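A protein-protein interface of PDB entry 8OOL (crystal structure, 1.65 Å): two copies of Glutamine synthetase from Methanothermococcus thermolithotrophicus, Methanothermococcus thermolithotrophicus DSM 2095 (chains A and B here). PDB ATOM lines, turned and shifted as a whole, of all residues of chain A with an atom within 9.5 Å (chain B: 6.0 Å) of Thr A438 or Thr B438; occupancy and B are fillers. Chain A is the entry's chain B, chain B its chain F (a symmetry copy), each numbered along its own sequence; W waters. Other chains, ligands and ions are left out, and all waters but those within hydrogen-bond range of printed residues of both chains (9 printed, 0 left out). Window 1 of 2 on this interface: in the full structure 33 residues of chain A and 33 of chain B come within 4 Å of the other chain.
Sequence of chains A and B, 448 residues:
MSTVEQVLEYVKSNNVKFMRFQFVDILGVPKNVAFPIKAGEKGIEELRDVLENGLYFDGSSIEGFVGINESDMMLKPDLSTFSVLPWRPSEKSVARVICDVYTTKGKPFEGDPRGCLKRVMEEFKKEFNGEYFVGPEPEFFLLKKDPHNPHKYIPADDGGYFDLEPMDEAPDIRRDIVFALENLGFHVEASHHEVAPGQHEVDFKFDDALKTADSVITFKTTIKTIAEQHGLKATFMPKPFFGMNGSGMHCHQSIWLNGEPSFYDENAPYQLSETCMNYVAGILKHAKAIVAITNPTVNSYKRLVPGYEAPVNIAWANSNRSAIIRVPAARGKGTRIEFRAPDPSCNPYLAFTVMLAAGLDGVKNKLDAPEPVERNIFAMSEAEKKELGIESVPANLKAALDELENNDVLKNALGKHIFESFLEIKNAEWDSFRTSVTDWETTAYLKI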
ATOM      1  N   MET A 237     -12.733  -1.412  32.409  1.00  0.00           N
ATOM      2  CA  MET A 237     -13.140  -2.726  31.854  1.00  0.00           C
ATOM      3  C   MET A 237     -12.056  -3.140  30.867  1.00  0.00           C
ATOM      4  O   MET A 237     -11.692  -2.324  30.014  1.00  0.00           O
ATOM      5  CB  MET A 237     -14.470  -2.609  31.107  1.00  0.00           C
ATOM      6  CG  MET A 237     -14.948  -3.896  30.490  1.00  0.00           C
ATOM      7  SD  MET A 237     -16.652  -3.697  29.929  1.00  0.00           S
ATOM      8  CE  MET A 237     -16.905  -5.260  29.091  1.00  0.00           C
ATOM      9  N   LYS A 239     -11.825  -5.141  28.245  1.00  0.00           N
ATOM     10  CA  LYS A 239     -12.132  -5.299  26.803  1.00  0.00           C
ATOM     11  C   LYS A 239     -13.585  -4.877  26.590  1.00  0.00           C
ATOM     12  O   LYS A 239     -14.445  -5.746  26.420  1.00  0.00           O
ATOM     13  CB  LYS A 239     -11.866  -6.736  26.350  1.00  0.00           C
ATOM     14  CG  LYS A 239     -12.016  -6.980  24.855  1.00  0.00           C
ATOM     15  CD  LYS A 239     -10.787  -6.607  24.058  1.00  0.00           C
ATOM     16  CE  LYS A 239     -10.929  -6.914  22.582  1.00  0.00           C
ATOM     17  NZ  LYS A 239      -9.648  -6.747  21.858  1.00  0.00           N
ATOM     18  N   PRO A 240     -13.871  -3.562  26.631  1.00  0.00           N
ATOM     19  CA  PRO A 240     -15.243  -3.085  26.505  1.00  0.00           C
ATOM     20  C   PRO A 240     -15.812  -3.262  25.092  1.00  0.00           C
ATOM     21  O   PRO A 240     -17.009  -3.347  24.956  1.00  0.00           O
ATOM     22  CB  PRO A 240     -15.118  -1.593  26.843  1.00  0.00           C
ATOM     23  CG  PRO A 240     -13.693  -1.243  26.483  1.00  0.00           C
ATOM     24  CD  PRO A 240     -12.896  -2.487  26.807  1.00  0.00           C
ATOM     25  N   PHE A 241     -14.938  -3.306  24.087  1.00  0.00           N
ATOM     26  CA  PHE A 241     -15.431  -3.381  22.692  1.00  0.00           C
ATOM     27  C   PHE A 241     -14.655  -4.422  21.882  1.00  0.00           C
ATOM     28  O   PHE A 241     -13.416  -4.385  21.861  1.00  0.00           O
ATOM     29  CB  PHE A 241     -15.352  -2.008  22.024  1.00  0.00           C
ATOM     30  CG  PHE A 241     -16.052  -0.906  22.777  1.00  0.00           C
ATOM     31  CD1 PHE A 241     -17.433  -0.806  22.765  1.00  0.00           C
ATOM     32  CD2 PHE A 241     -15.329   0.027  23.501  1.00  0.00           C
ATOM     33  CE1 PHE A 241     -18.075   0.205  23.459  1.00  0.00           C
ATOM     34  CE2 PHE A 241     -15.974   1.036  24.196  1.00  0.00           C
ATOM     35  CZ  PHE A 241     -17.345   1.124  24.174  1.00  0.00           C
ATOM     36  N   PHE A 242     -15.389  -5.312  21.221  1.00  0.00           N
ATOM     37  CA  PHE A 242     -14.728  -6.289  20.328  1.00  0.00           C
ATOM     38  C   PHE A 242     -14.207  -5.547  19.098  1.00  0.00           C
ATOM     39  O   PHE A 242     -14.830  -4.564  18.683  1.00  0.00           O
ATOM     40  CB  PHE A 242     -15.707  -7.387  19.908  1.00  0.00           C
ATOM     41  CG  PHE A 242     -15.113  -8.415  18.981  1.00  0.00           C
ATOM     42  CD1 PHE A 242     -14.362  -9.467  19.478  1.00  0.00           C
ATOM     43  CD2 PHE A 242     -15.290  -8.320  17.611  1.00  0.00           C
ATOM     44  CE1 PHE A 242     -13.808 -10.406  18.625  1.00  0.00           C
ATOM     45  CE2 PHE A 242     -14.737  -9.262  16.759  1.00  0.00           C
ATOM     46  CZ  PHE A 242     -13.996 -10.302  17.268  1.00  0.00           C
ATOM     47  N   VAL A 298     -14.189 -11.952  34.143  1.00  0.00           N
ATOM     48  CA  VAL A 298     -14.451 -12.792  32.987  1.00  0.00           C
ATOM     49  C   VAL A 298     -13.888 -12.072  31.736  1.00  0.00           C
ATOM     50  O   VAL A 298     -13.264 -12.678  30.886  1.00  0.00           O
ATOM     51  CB  VAL A 298     -15.987 -12.992  32.831  1.00  0.00           C
ATOM     52  CG1 VAL A 298     -16.321 -13.547  31.448  1.00  0.00           C
ATOM     53  CG2 VAL A 298     -16.517 -13.919  33.932  1.00  0.00           C
ATOM     54  N   ASN A 299     -14.141 -10.760  31.661  1.00  0.00           N
ATOM     55  CA  ASN A 299     -13.766  -9.907  30.518  1.00  0.00           C
ATOM     56  C   ASN A 299     -12.270  -9.758  30.320  1.00  0.00           C
ATOM     57  O   ASN A 299     -11.803  -9.528  29.199  1.00  0.00           O
ATOM     58  CB  ASN A 299     -14.471  -8.582  30.647  1.00  0.00           C
ATOM     59  CG  ASN A 299     -14.271  -7.625  29.490  1.00  0.00           C
ATOM     60  OD1 ASN A 299     -13.609  -6.598  29.664  1.00  0.00           O
ATOM     61  ND2 ASN A 299     -14.829  -7.931  28.318  1.00  0.00           N
ATOM     62  N   LYS A 302     -10.967 -11.694  27.463  1.00  0.00           N
ATOM     63  CA  LYS A 302     -11.321 -11.314  26.080  1.00  0.00           C
ATOM     64  C   LYS A 302     -10.183 -10.410  25.567  1.00  0.00           C
ATOM     65  O   LYS A 302     -10.069 -10.160  24.365  1.00  0.00           O
ATOM     66  CB  LYS A 302     -12.687 -10.622  26.016  1.00  0.00           C
ATOM     67  CG  LYS A 302     -13.823 -11.671  25.929  1.00  0.00           C
ATOM     68  CD  LYS A 302     -14.074 -12.535  27.161  1.00  0.00           C
ATOM     69  CE  LYS A 302     -15.090 -13.654  26.919  1.00  0.00           C
ATOM     70  NZ  LYS A 302     -16.387 -13.161  26.384  1.00  0.00           N
ATOM     71  N   SER A 432     -22.375 -17.104  37.530  1.00  0.00           N
ATOM     72  CA  SER A 432     -23.348 -16.108  37.012  1.00  0.00           C
ATOM     73  C   SER A 432     -23.156 -15.971  35.499  1.00  0.00           C
ATOM     74  O   SER A 432     -24.152 -16.068  34.765  1.00  0.00           O
ATOM     75  CB  SER A 432     -23.205 -14.783  37.709  1.00  0.00           C
ATOM     76  OG  SER A 432     -24.023 -13.801  37.092  1.00  0.00           O
ATOM     77  N   PHE A 433     -21.910 -15.760  35.060  1.00  0.00           N
ATOM     78  CA  PHE A 433     -21.652 -15.621  33.626  1.00  0.00           C
ATOM     79  C   PHE A 433     -21.983 -16.903  32.869  1.00  0.00           C
ATOM     80  O   PHE A 433     -22.624 -16.857  31.809  1.00  0.00           O
ATOM     81  CB  PHE A 433     -20.148 -15.293  33.415  1.00  0.00           C
ATOM     82  CG  PHE A 433     -19.723 -15.323  31.957  1.00  0.00           C
ATOM     83  CD1 PHE A 433     -20.266 -14.428  31.043  1.00  0.00           C
ATOM     84  CD2 PHE A 433     -18.775 -16.239  31.512  1.00  0.00           C
ATOM     85  CE1 PHE A 433     -19.872 -14.459  29.691  1.00  0.00           C
ATOM     86  CE2 PHE A 433     -18.375 -16.267  30.173  1.00  0.00           C
ATOM     87  CZ  PHE A 433     -18.922 -15.370  29.272  1.00  0.00           C
ATOM     88  N   ARG A 434     -21.540 -18.048  33.396  1.00  0.00           N
ATOM     89  CA  ARG A 434     -21.701 -19.333  32.657  1.00  0.00           C
ATOM     90  C   ARG A 434     -23.178 -19.716  32.486  1.00  0.00           C
ATOM     91  O   ARG A 434     -23.477 -20.424  31.511  1.00  0.00           O
ATOM     92  CB  ARG A 434     -20.914 -20.449  33.352  1.00  0.00           C
ATOM     93  CG  ARG A 434     -21.730 -21.276  34.332  1.00  0.00           C
ATOM     94  CD  ARG A 434     -20.824 -22.199  35.123  1.00  0.00           C
ATOM     95  NE  ARG A 434     -21.562 -23.093  36.002  1.00  0.00           N
ATOM     96  CZ  ARG A 434     -22.185 -24.195  35.602  1.00  0.00           C
ATOM     97  NH1 ARG A 434     -21.981 -24.667  34.386  1.00  0.00           N
ATOM     98  NH2 ARG A 434     -23.011 -24.823  36.422  1.00  0.00           N
ATOM     99  N   THR A 435     -24.055 -19.302  33.401  1.00  0.00           N
ATOM    100  CA  THR A 435     -25.467 -19.729  33.284  1.00  0.00           C
ATOM    101  C   THR A 435     -26.314 -18.662  32.568  1.00  0.00           C
ATOM    102  O   THR A 435     -27.486 -18.909  32.258  1.00  0.00           O
ATOM    103  CB  THR A 435     -26.052 -20.013  34.679  1.00  0.00           C
ATOM    104  OG1 THR A 435     -26.004 -18.809  35.460  1.00  0.00           O
ATOM    105  CG2 THR A 435     -25.325 -21.153  35.379  1.00  0.00           C
ATOM    106  N   SER A 436     -25.722 -17.488  32.294  1.00  0.00           N
ATOM    107  CA  SER A 436     -26.453 -16.414  31.627  1.00  0.00           C
ATOM    108  C   SER A 436     -26.713 -16.752  30.165  1.00  0.00           C
ATOM    109  O   SER A 436     -26.034 -17.596  29.602  1.00  0.00           O
ATOM    110  CB  SER A 436     -25.639 -15.122  31.676  1.00  0.00           C
ATOM    111  OG  SER A 436     -24.565 -15.213  30.756  1.00  0.00           O
ATOM    112  N   VAL A 437     -27.704 -16.102  29.546  1.00  0.00           N
ATOM    113  CA  VAL A 437     -27.947 -16.289  28.119  1.00  0.00           C
ATOM    114  C   VAL A 437     -27.440 -15.001  27.510  1.00  0.00           C
ATOM    115  O   VAL A 437     -27.986 -13.933  27.778  1.00  0.00           O
ATOM    116  CB  VAL A 437     -29.426 -16.521  27.764  1.00  0.00           C
ATOM    117  CG1 VAL A 437     -29.584 -16.558  26.247  1.00  0.00           C
ATOM    118  CG2 VAL A 437     -29.931 -17.823  28.409  1.00  0.00           C
ATOM    119  N   THR A 438     -26.377 -15.074  26.721  1.00  0.00           N
ATOM    120  CA  THR A 438     -25.777 -13.863  26.164  1.00  0.00           C
ATOM    121  C   THR A 438     -26.336 -13.404  24.844  1.00  0.00           C
ATOM    122  O   THR A 438     -26.990 -14.166  24.094  1.00  0.00           O
ATOM    123  CB  THR A 438     -24.246 -14.058  26.023  1.00  0.00           C
ATOM    124  OG1 THR A 438     -24.004 -15.010  24.972  1.00  0.00           O
ATOM    125  CG2 THR A 438     -23.595 -14.490  27.328  1.00  0.00           C
ATOM    126  N   ASP A 439     -26.049 -12.139  24.520  1.00  0.00           N
ATOM    127  CA  ASP A 439     -26.490 -11.581  23.215  1.00  0.00           C
ATOM    128  C   ASP A 439     -25.848 -12.379  22.072  1.00  0.00           C
ATOM    129  O   ASP A 439     -26.510 -12.588  21.050  1.00  0.00           O
ATOM    130  CB  ASP A 439     -26.200 -10.080  23.122  1.00  0.00           C
ATOM    131  CG  ASP A 439     -24.780  -9.677  23.478  1.00  0.00           C
ATOM    132  OD1 ASP A 439     -24.011 -10.547  23.919  1.00  0.00           O
ATOM    133  OD2 ASP A 439     -24.458  -8.488  23.309  1.00  0.00           O
ATOM    134  N   TRP A 440     -24.603 -12.813  22.264  1.00  0.00           N
ATOM    135  CA  TRP A 440     -23.917 -13.604  21.213  1.00  0.00           C
ATOM    136  C   TRP A 440     -24.760 -14.839  20.887  1.00  0.00           C
ATOM    137  O   TRP A 440     -24.926 -15.141  19.700  1.00  0.00           O
ATOM    138  CB  TRP A 440     -22.508 -14.002  21.662  1.00  0.00           C
ATOM    139  CG  TRP A 440     -21.720 -14.674  20.581  1.00  0.00           C
ATOM    140  CD1 TRP A 440     -20.813 -14.092  19.744  1.00  0.00           C
ATOM    141  CD2 TRP A 440     -21.780 -16.059  20.203  1.00  0.00           C
ATOM    142  NE1 TRP A 440     -20.302 -15.018  18.878  1.00  0.00           N
ATOM    143  CE2 TRP A 440     -20.876 -16.235  19.136  1.00  0.00           C
ATOM    144  CE3 TRP A 440     -22.504 -17.165  20.662  1.00  0.00           C
ATOM    145  CZ2 TRP A 440     -20.680 -17.471  18.524  1.00  0.00           C
ATOM    146  CZ3 TRP A 440     -22.310 -18.386  20.056  1.00  0.00           C
ATOM    147  CH2 TRP A 440     -21.410 -18.534  19.003  1.00  0.00           C
ATOM    148  N   GLU A 441     -25.265 -15.513  21.917  1.00  0.00           N
ATOM    149  CA  GLU A 441     -26.041 -16.763  21.704  1.00  0.00           C
ATOM    150  C   GLU A 441     -27.357 -16.448  20.982  1.00  0.00           C
ATOM    151  O   GLU A 441     -27.723 -17.189  20.070  1.00  0.00           O
ATOM    152  CB  GLU A 441     -26.296 -17.444  23.047  1.00  0.00           C
ATOM    153  CG  GLU A 441     -25.028 -17.905  23.735  1.00  0.00           C
ATOM    154  CD  GLU A 441     -25.228 -18.205  25.208  1.00  0.00           C
ATOM    155  OE1 GLU A 441     -24.777 -17.398  26.039  1.00  0.00           O
ATOM    156  OE2 GLU A 441     -25.846 -19.240  25.515  1.00  0.00           O
ATOM    157  N   THR A 442     -28.031 -15.381  21.405  1.00  0.00           N
ATOM    158  CA  THR A 442     -29.315 -15.002  20.763  1.00  0.00           C
ATOM    159  C   THR A 442     -29.054 -14.708  19.280  1.00  0.00           C
ATOM    160  O   THR A 442     -29.835 -15.162  18.436  1.00  0.00           O
ATOM    161  CB  THR A 442     -29.971 -13.834  21.511  1.00  0.00           C
ATOM    162  OG1 THR A 442     -30.359 -14.304  22.801  1.00  0.00           O
ATOM    163  CG2 THR A 442     -31.168 -13.267  20.781  1.00  0.00           C
ATOM    164  N   THR A 443     -27.978 -13.981  18.993  1.00  0.00           N
ATOM    165  CA  THR A 443     -27.668 -13.623  17.587  1.00  0.00           C
ATOM    166  C   THR A 443     -27.347 -14.899  16.803  1.00  0.00           C
ATOM    167  O   THR A 443     -27.777 -15.013  15.652  1.00  0.00           O
ATOM    168  CB  THR A 443     -26.524 -12.599  17.534  1.00  0.00           C
ATOM    169  OG1 THR A 443     -26.953 -11.396  18.173  1.00  0.00           O
ATOM    170  CG2 THR A 443     -26.061 -12.303  16.124  1.00  0.00           C
ATOM    171  N   ALA A 444     -26.631 -15.831  17.424  1.00  0.00           N
ATOM    172  CA  ALA A 444     -26.187 -17.043  16.700  1.00  0.00           C
ATOM    173  C   ALA A 444     -27.273 -18.115  16.573  1.00  0.00           C
ATOM    174  O   ALA A 444     -27.271 -18.811  15.551  1.00  0.00           O
ATOM    175  CB  ALA A 444     -25.000 -17.626  17.430  1.00  0.00           C
ATOM    176  N   TYR A 445     -28.176 -18.233  17.550  1.00  0.00           N
ATOM    177  CA  TYR A 445     -29.081 -19.418  17.547  1.00  0.00           C
ATOM    178  C   TYR A 445     -30.590 -19.141  17.474  1.00  0.00           C
ATOM    179  O   TYR A 445     -31.329 -20.119  17.345  1.00  0.00           O
ATOM    180  CB  TYR A 445     -28.782 -20.249  18.798  1.00  0.00           C
ATOM    181  CG  TYR A 445     -27.331 -20.619  18.962  1.00  0.00           C
ATOM    182  CD1 TYR A 445     -26.671 -21.347  17.988  1.00  0.00           C
ATOM    183  CD2 TYR A 445     -26.615 -20.238  20.083  1.00  0.00           C
ATOM    184  CE1 TYR A 445     -25.338 -21.693  18.125  1.00  0.00           C
ATOM    185  CE2 TYR A 445     -25.282 -20.577  20.238  1.00  0.00           C
ATOM    186  CZ  TYR A 445     -24.640 -21.307  19.254  1.00  0.00           C
ATOM    187  OH  TYR A 445     -23.320 -21.648  19.395  1.00  0.00           O
ATOM    188  N   LEU A 446     -31.044 -17.896  17.568  1.00  0.00           N
ATOM    189  CA  LEU A 446     -32.524 -17.716  17.563  1.00  0.00           C
ATOM    190  C   LEU A 446     -33.102 -18.298  16.264  1.00  0.00           C
ATOM    191  O   LEU A 446     -34.222 -18.825  16.312  1.00  0.00           O
ATOM    192  CB  LEU A 446     -32.879 -16.239  17.755  1.00  0.00           C
ATOM    193  CG  LEU A 446     -34.246 -15.977  18.384  1.00  0.00           C
ATOM    194  CD1 LEU A 446     -34.344 -16.621  19.756  1.00  0.00           C
ATOM    195  CD2 LEU A 446     -34.523 -14.485  18.473  1.00  0.00           C
ATOM    196  N   MET B 237     -33.789 -22.891  19.659  1.00  0.00           N
ATOM    197  CA  MET B 237     -32.643 -22.476  20.488  1.00  0.00           C
ATOM    198  C   MET B 237     -32.873 -23.141  21.859  1.00  0.00           C
ATOM    199  O   MET B 237     -33.946 -23.031  22.423  1.00  0.00           O
ATOM    200  CB  MET B 237     -32.694 -20.953  20.652  1.00  0.00           C
ATOM    201  CG  MET B 237     -31.556 -20.422  21.526  1.00  0.00           C
ATOM    202  SD  MET B 237     -31.518 -18.629  21.398  1.00  0.00           S
ATOM    203  CE  MET B 237     -30.119 -18.273  22.542  1.00  0.00           C
ATOM    204  N   ASN B 299     -25.113 -22.460  23.481  1.00  0.00           N
ATOM    205  CA  ASN B 299     -26.346 -22.237  24.255  1.00  0.00           C
ATOM    206  C   ASN B 299     -26.929 -23.513  24.853  1.00  0.00           C
ATOM    207  O   ASN B 299     -27.609 -23.454  25.886  1.00  0.00           O
ATOM    208  CB  ASN B 299     -27.343 -21.481  23.388  1.00  0.00           C
ATOM    209  CG  ASN B 299     -28.627 -21.110  24.092  1.00  0.00           C
ATOM    210  OD1 ASN B 299     -29.674 -21.660  23.738  1.00  0.00           O
ATOM    211  ND2 ASN B 299     -28.557 -20.194  25.069  1.00  0.00           N
ATOM    212  N   LYS B 302     -26.392 -23.860  28.461  1.00  0.00           N
ATOM    213  CA  LYS B 302     -27.079 -22.942  29.402  1.00  0.00           C
ATOM    214  C   LYS B 302     -28.369 -23.668  29.870  1.00  0.00           C
ATOM    215  O   LYS B 302     -28.994 -23.276  30.854  1.00  0.00           O
ATOM    216  CB  LYS B 302     -27.347 -21.581  28.764  1.00  0.00           C
ATOM    217  CG  LYS B 302     -26.122 -20.667  28.903  1.00  0.00           C
ATOM    218  CD  LYS B 302     -24.903 -21.014  28.068  1.00  0.00           C
ATOM    219  CE  LYS B 302     -23.669 -20.151  28.359  1.00  0.00           C
ATOM    220  NZ  LYS B 302     -23.959 -18.672  28.320  1.00  0.00           N
ATOM    221  N   PHE B 433     -17.466 -17.297  20.026  1.00  0.00           N
ATOM    222  CA  PHE B 433     -18.118 -16.958  21.282  1.00  0.00           C
ATOM    223  C   PHE B 433     -17.088 -16.522  22.338  1.00  0.00           C
ATOM    224  O   PHE B 433     -17.291 -15.512  23.025  1.00  0.00           O
ATOM    225  CB  PHE B 433     -18.861 -18.207  21.826  1.00  0.00           C
ATOM    226  CG  PHE B 433     -19.419 -18.049  23.233  1.00  0.00           C
ATOM    227  CD1 PHE B 433     -20.385 -17.080  23.511  1.00  0.00           C
ATOM    228  CD2 PHE B 433     -18.949 -18.839  24.277  1.00  0.00           C
ATOM    229  CE1 PHE B 433     -20.882 -16.916  24.825  1.00  0.00           C
ATOM    230  CE2 PHE B 433     -19.447 -18.692  25.573  1.00  0.00           C
ATOM    231  CZ  PHE B 433     -20.407 -17.732  25.841  1.00  0.00           C
ATOM    232  N   SER B 436     -15.765 -12.974  21.880  1.00  0.00           N
ATOM    233  CA  SER B 436     -16.771 -11.922  21.818  1.00  0.00           C
ATOM    234  C   SER B 436     -16.847 -11.142  23.124  1.00  0.00           C
ATOM    235  O   SER B 436     -16.411 -11.641  24.150  1.00  0.00           O
ATOM    236  CB  SER B 436     -18.143 -12.539  21.540  1.00  0.00           C
ATOM    237  OG  SER B 436     -18.631 -13.145  22.728  1.00  0.00           O
ATOM    238  N   VAL B 437     -17.391  -9.926  23.071  1.00  0.00           N
ATOM    239  CA  VAL B 437     -17.636  -9.167  24.329  1.00  0.00           C
ATOM    240  C   VAL B 437     -19.143  -9.252  24.570  1.00  0.00           C
ATOM    241  O   VAL B 437     -19.887  -8.700  23.752  1.00  0.00           O
ATOM    242  CB  VAL B 437     -17.143  -7.711  24.246  1.00  0.00           C
ATOM    243  CG1 VAL B 437     -17.557  -6.919  25.477  1.00  0.00           C
ATOM    244  CG2 VAL B 437     -15.638  -7.645  24.050  1.00  0.00           C
ATOM    245  N   THR B 438     -19.561  -9.936  25.632  1.00  0.00           N
ATOM    246  CA  THR B 438     -21.009 -10.187  25.845  1.00  0.00           C
ATOM    247  C   THR B 438     -21.701  -9.061  26.610  1.00  0.00           C
ATOM    248  O   THR B 438     -21.017  -8.304  27.312  1.00  0.00           O
ATOM    249  CB  THR B 438     -21.219 -11.503  26.606  1.00  0.00           C
ATOM    250  OG1 THR B 438     -20.661 -11.369  27.912  1.00  0.00           O
ATOM    251  CG2 THR B 438     -20.602 -12.686  25.893  1.00  0.00           C
ATOM    252  N   ASP B 439     -23.027  -9.007  26.491  1.00  0.00           N
ATOM    253  CA  ASP B 439     -23.810  -8.005  27.253  1.00  0.00           C
ATOM    254  C   ASP B 439     -23.609  -8.253  28.752  1.00  0.00           C
ATOM    255  O   ASP B 439     -23.556  -7.281  29.511  1.00  0.00           O
ATOM    256  CB  ASP B 439     -25.282  -8.045  26.838  1.00  0.00           C
ATOM    257  CG  ASP B 439     -25.921  -9.424  26.864  1.00  0.00           C
ATOM    258  OD1 ASP B 439     -25.195 -10.412  27.065  1.00  0.00           O
ATOM    259  OD2 ASP B 439     -27.151  -9.494  26.678  1.00  0.00           O
ATOM    260  N   TRP B 440     -23.497  -9.523  29.146  1.00  0.00           N
ATOM    261  CA  TRP B 440     -23.269  -9.852  30.578  1.00  0.00           C
ATOM    262  C   TRP B 440     -22.023  -9.117  31.075  1.00  0.00           C
ATOM    263  O   TRP B 440     -22.073  -8.564  32.175  1.00  0.00           O
ATOM    264  CB  TRP B 440     -23.123 -11.364  30.776  1.00  0.00           C
ATOM    265  CG  TRP B 440     -23.042 -11.754  32.219  1.00  0.00           C
ATOM    266  CD1 TRP B 440     -24.065 -12.181  33.014  1.00  0.00           C
ATOM    267  CD2 TRP B 440     -21.868 -11.734  33.049  1.00  0.00           C
ATOM    268  NE1 TRP B 440     -23.608 -12.433  34.279  1.00  0.00           N
ATOM    269  CE2 TRP B 440     -22.265 -12.170  34.330  1.00  0.00           C
ATOM    270  CE3 TRP B 440     -20.528 -11.396  32.837  1.00  0.00           C
ATOM    271  CZ2 TRP B 440     -21.367 -12.274  35.390  1.00  0.00           C
ATOM    272  CZ3 TRP B 440     -19.641 -11.499  33.884  1.00  0.00           C
ATOM    273  CH2 TRP B 440     -20.058 -11.933  35.142  1.00  0.00           C
ATOM    274  N   GLU B 441     -20.958  -9.121  30.273  1.00  0.00           N
ATOM    275  CA  GLU B 441     -19.679  -8.494  30.693  1.00  0.00           C
ATOM    276  C   GLU B 441     -19.832  -6.973  30.775  1.00  0.00           C
ATOM    277  O   GLU B 441     -19.314  -6.379  31.723  1.00  0.00           O
ATOM    278  CB  GLU B 441     -18.577  -8.870  29.702  1.00  0.00           C
ATOM    279  CG  GLU B 441     -18.260 -10.349  29.687  1.00  0.00           C
ATOM    280  CD  GLU B 441     -17.458 -10.780  28.472  1.00  0.00           C
ATOM    281  OE1 GLU B 441     -18.043 -11.403  27.573  1.00  0.00           O
ATOM    282  OE2 GLU B 441     -16.251 -10.475  28.431  1.00  0.00           O
ATOM    283  N   THR B 442     -20.511  -6.386  29.793  1.00  0.00           N
ATOM    284  CA  THR B 442     -20.726  -4.917  29.802  1.00  0.00           C
ATOM    285  C   THR B 442     -21.528  -4.551  31.056  1.00  0.00           C
ATOM    286  O   THR B 442     -21.167  -3.581  31.732  1.00  0.00           O
ATOM    287  CB  THR B 442     -21.379  -4.449  28.495  1.00  0.00           C
ATOM    288  OG1 THR B 442     -20.450  -4.687  27.438  1.00  0.00           O
ATOM    289  CG2 THR B 442     -21.780  -2.992  28.520  1.00  0.00           C
ATOM    290  N   THR B 443     -22.568  -5.330  31.344  1.00  0.00           N
ATOM    291  CA  THR B 443     -23.416  -5.047  32.531  1.00  0.00           C
ATOM    292  C   THR B 443     -22.581  -5.199  33.806  1.00  0.00           C
ATOM    293  O   THR B 443     -22.744  -4.380  34.715  1.00  0.00           O
ATOM    294  CB  THR B 443     -24.661  -5.948  32.522  1.00  0.00           C
ATOM    295  OG1 THR B 443     -25.457  -5.623  31.383  1.00  0.00           O
ATOM    296  CG2 THR B 443     -25.487  -5.822  33.783  1.00  0.00           C
HETATM  297  O   HOH W   1     -17.781 -15.652  25.861  1.00  0.00           O
HETATM  298  O   HOH W   2     -21.584 -17.493  29.264  1.00  0.00           O
HETATM  299  O   HOH W   3     -26.266 -11.961  29.622  1.00  0.00           O
HETATM  300  O   HOH W   4     -19.021  -2.583  26.575  1.00  0.00           O
HETATM  301  O   HOH W   5     -28.757 -11.603  26.757  1.00  0.00           O
HETATM  302  O   HOH W   6     -29.001 -21.071  32.540  1.00  0.00           O
HETATM  303  O   HOH W   7     -22.098  -7.261  23.475  1.00  0.00           O
HETATM  304  O   HOH W   8     -26.476 -12.275  35.441  1.00  0.00           O
HETATM  305  O   HOH W   9     -21.498 -10.692  21.950  1.00  0.00           O
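N of Asp B439 sits at hydrogen-bond distance from OD1 of Asp A439 (3.2 Å). The indole nitrogen (NE1) of Trp B440 sits at hydrogen-bond distance from the side-chain hydroxyl (OG) of Ser A432, at 3.2 Å. NZ of Lys B302 sits at hydrogen-bond distance from O of Ser A436 (2.7 Å). OE2 of Glu A441 lies within hydrogen-bond range of ND2 of Asn B299 (2.9 Å). OE1 of Glu B441 is in salt-bridge range of NZ of Lys A302 (2.7 Å). The side-chain carboxylate (OE1) of Glu A441 lies within salt-bridge range of the side-chain amino group (NZ) of Lys B302 (2.7 Å). NZ of Lys A302 sits at hydrogen-bond distance from O of Ser B436, 2.7 Å away. ND2 of Asn A299 is in hydrogen-bond range of OE2 of Glu B441 (2.9 Å).
OD1 of Asn A299 is in hydrogen-bond range of N of Lys A239 (2.7 Å). The backbone carbonyl oxygen (O) of Phe A433 lies within hydrogen-bond range of the side-chain hydroxyl (OG) of Ser A436, 2.8 Å away.
Thr B438 touches just these residues of chain A: Phe A433 (3.7 Å), Thr A438 (3.8 Å) and Asp A439 (3.6 Å). Of chain A, only Met A237 (3.7 Å), Asn A299 (2.9 Å) and Lys A302 (2.7 Å) come within 4 Å of Glu B441. Printed residues of chain A within 4 Å of Val B437: Lys A239 (3.3 Å), Pro A240 (3.7 Å) and Phe A242 (3.7 Å). Of the printed residues of chain B, Leu A446 touches Met B237. The nearest residue of chain A that does not touch Thr B438 is Lys A302 (4.3 Å).
Of the 23 printed residues of chain A, 19 touch a printed residue of chain B. Along chain A the printed residues that touch a printed residue of chain B span positions 237 to 446. Hydrophobic or aromatic side chains of chain B within 4 Å of the printed part of chain A: Met B237, Phe B433, Val B437 and Trp B440. Among the printed residues, 30 pairs touch across the chains. Among the printed residues, Asp or Glu carboxylates within 4 Å of a Lys or Arg side-chain nitrogen of the other chain: Lys A302 with Glu B441 and Glu A441 with Lys B302.
Phe A433 touches Thr B438, and with the chains exchanged Thr A438 touches Phe B433. Of the 30 pairs that touch across the chains among the printed residues, 20 have their exchanged pair printed and touching as well.
Water W5 lies within hydrogen-bond range of the side-chain carboxylate (OD2) of Asp B439 and the backbone carbonyl oxygen (O) of Val A437. Water W6 lies within hydrogen-bond range of O of Thr A435 and O of Lys B302.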
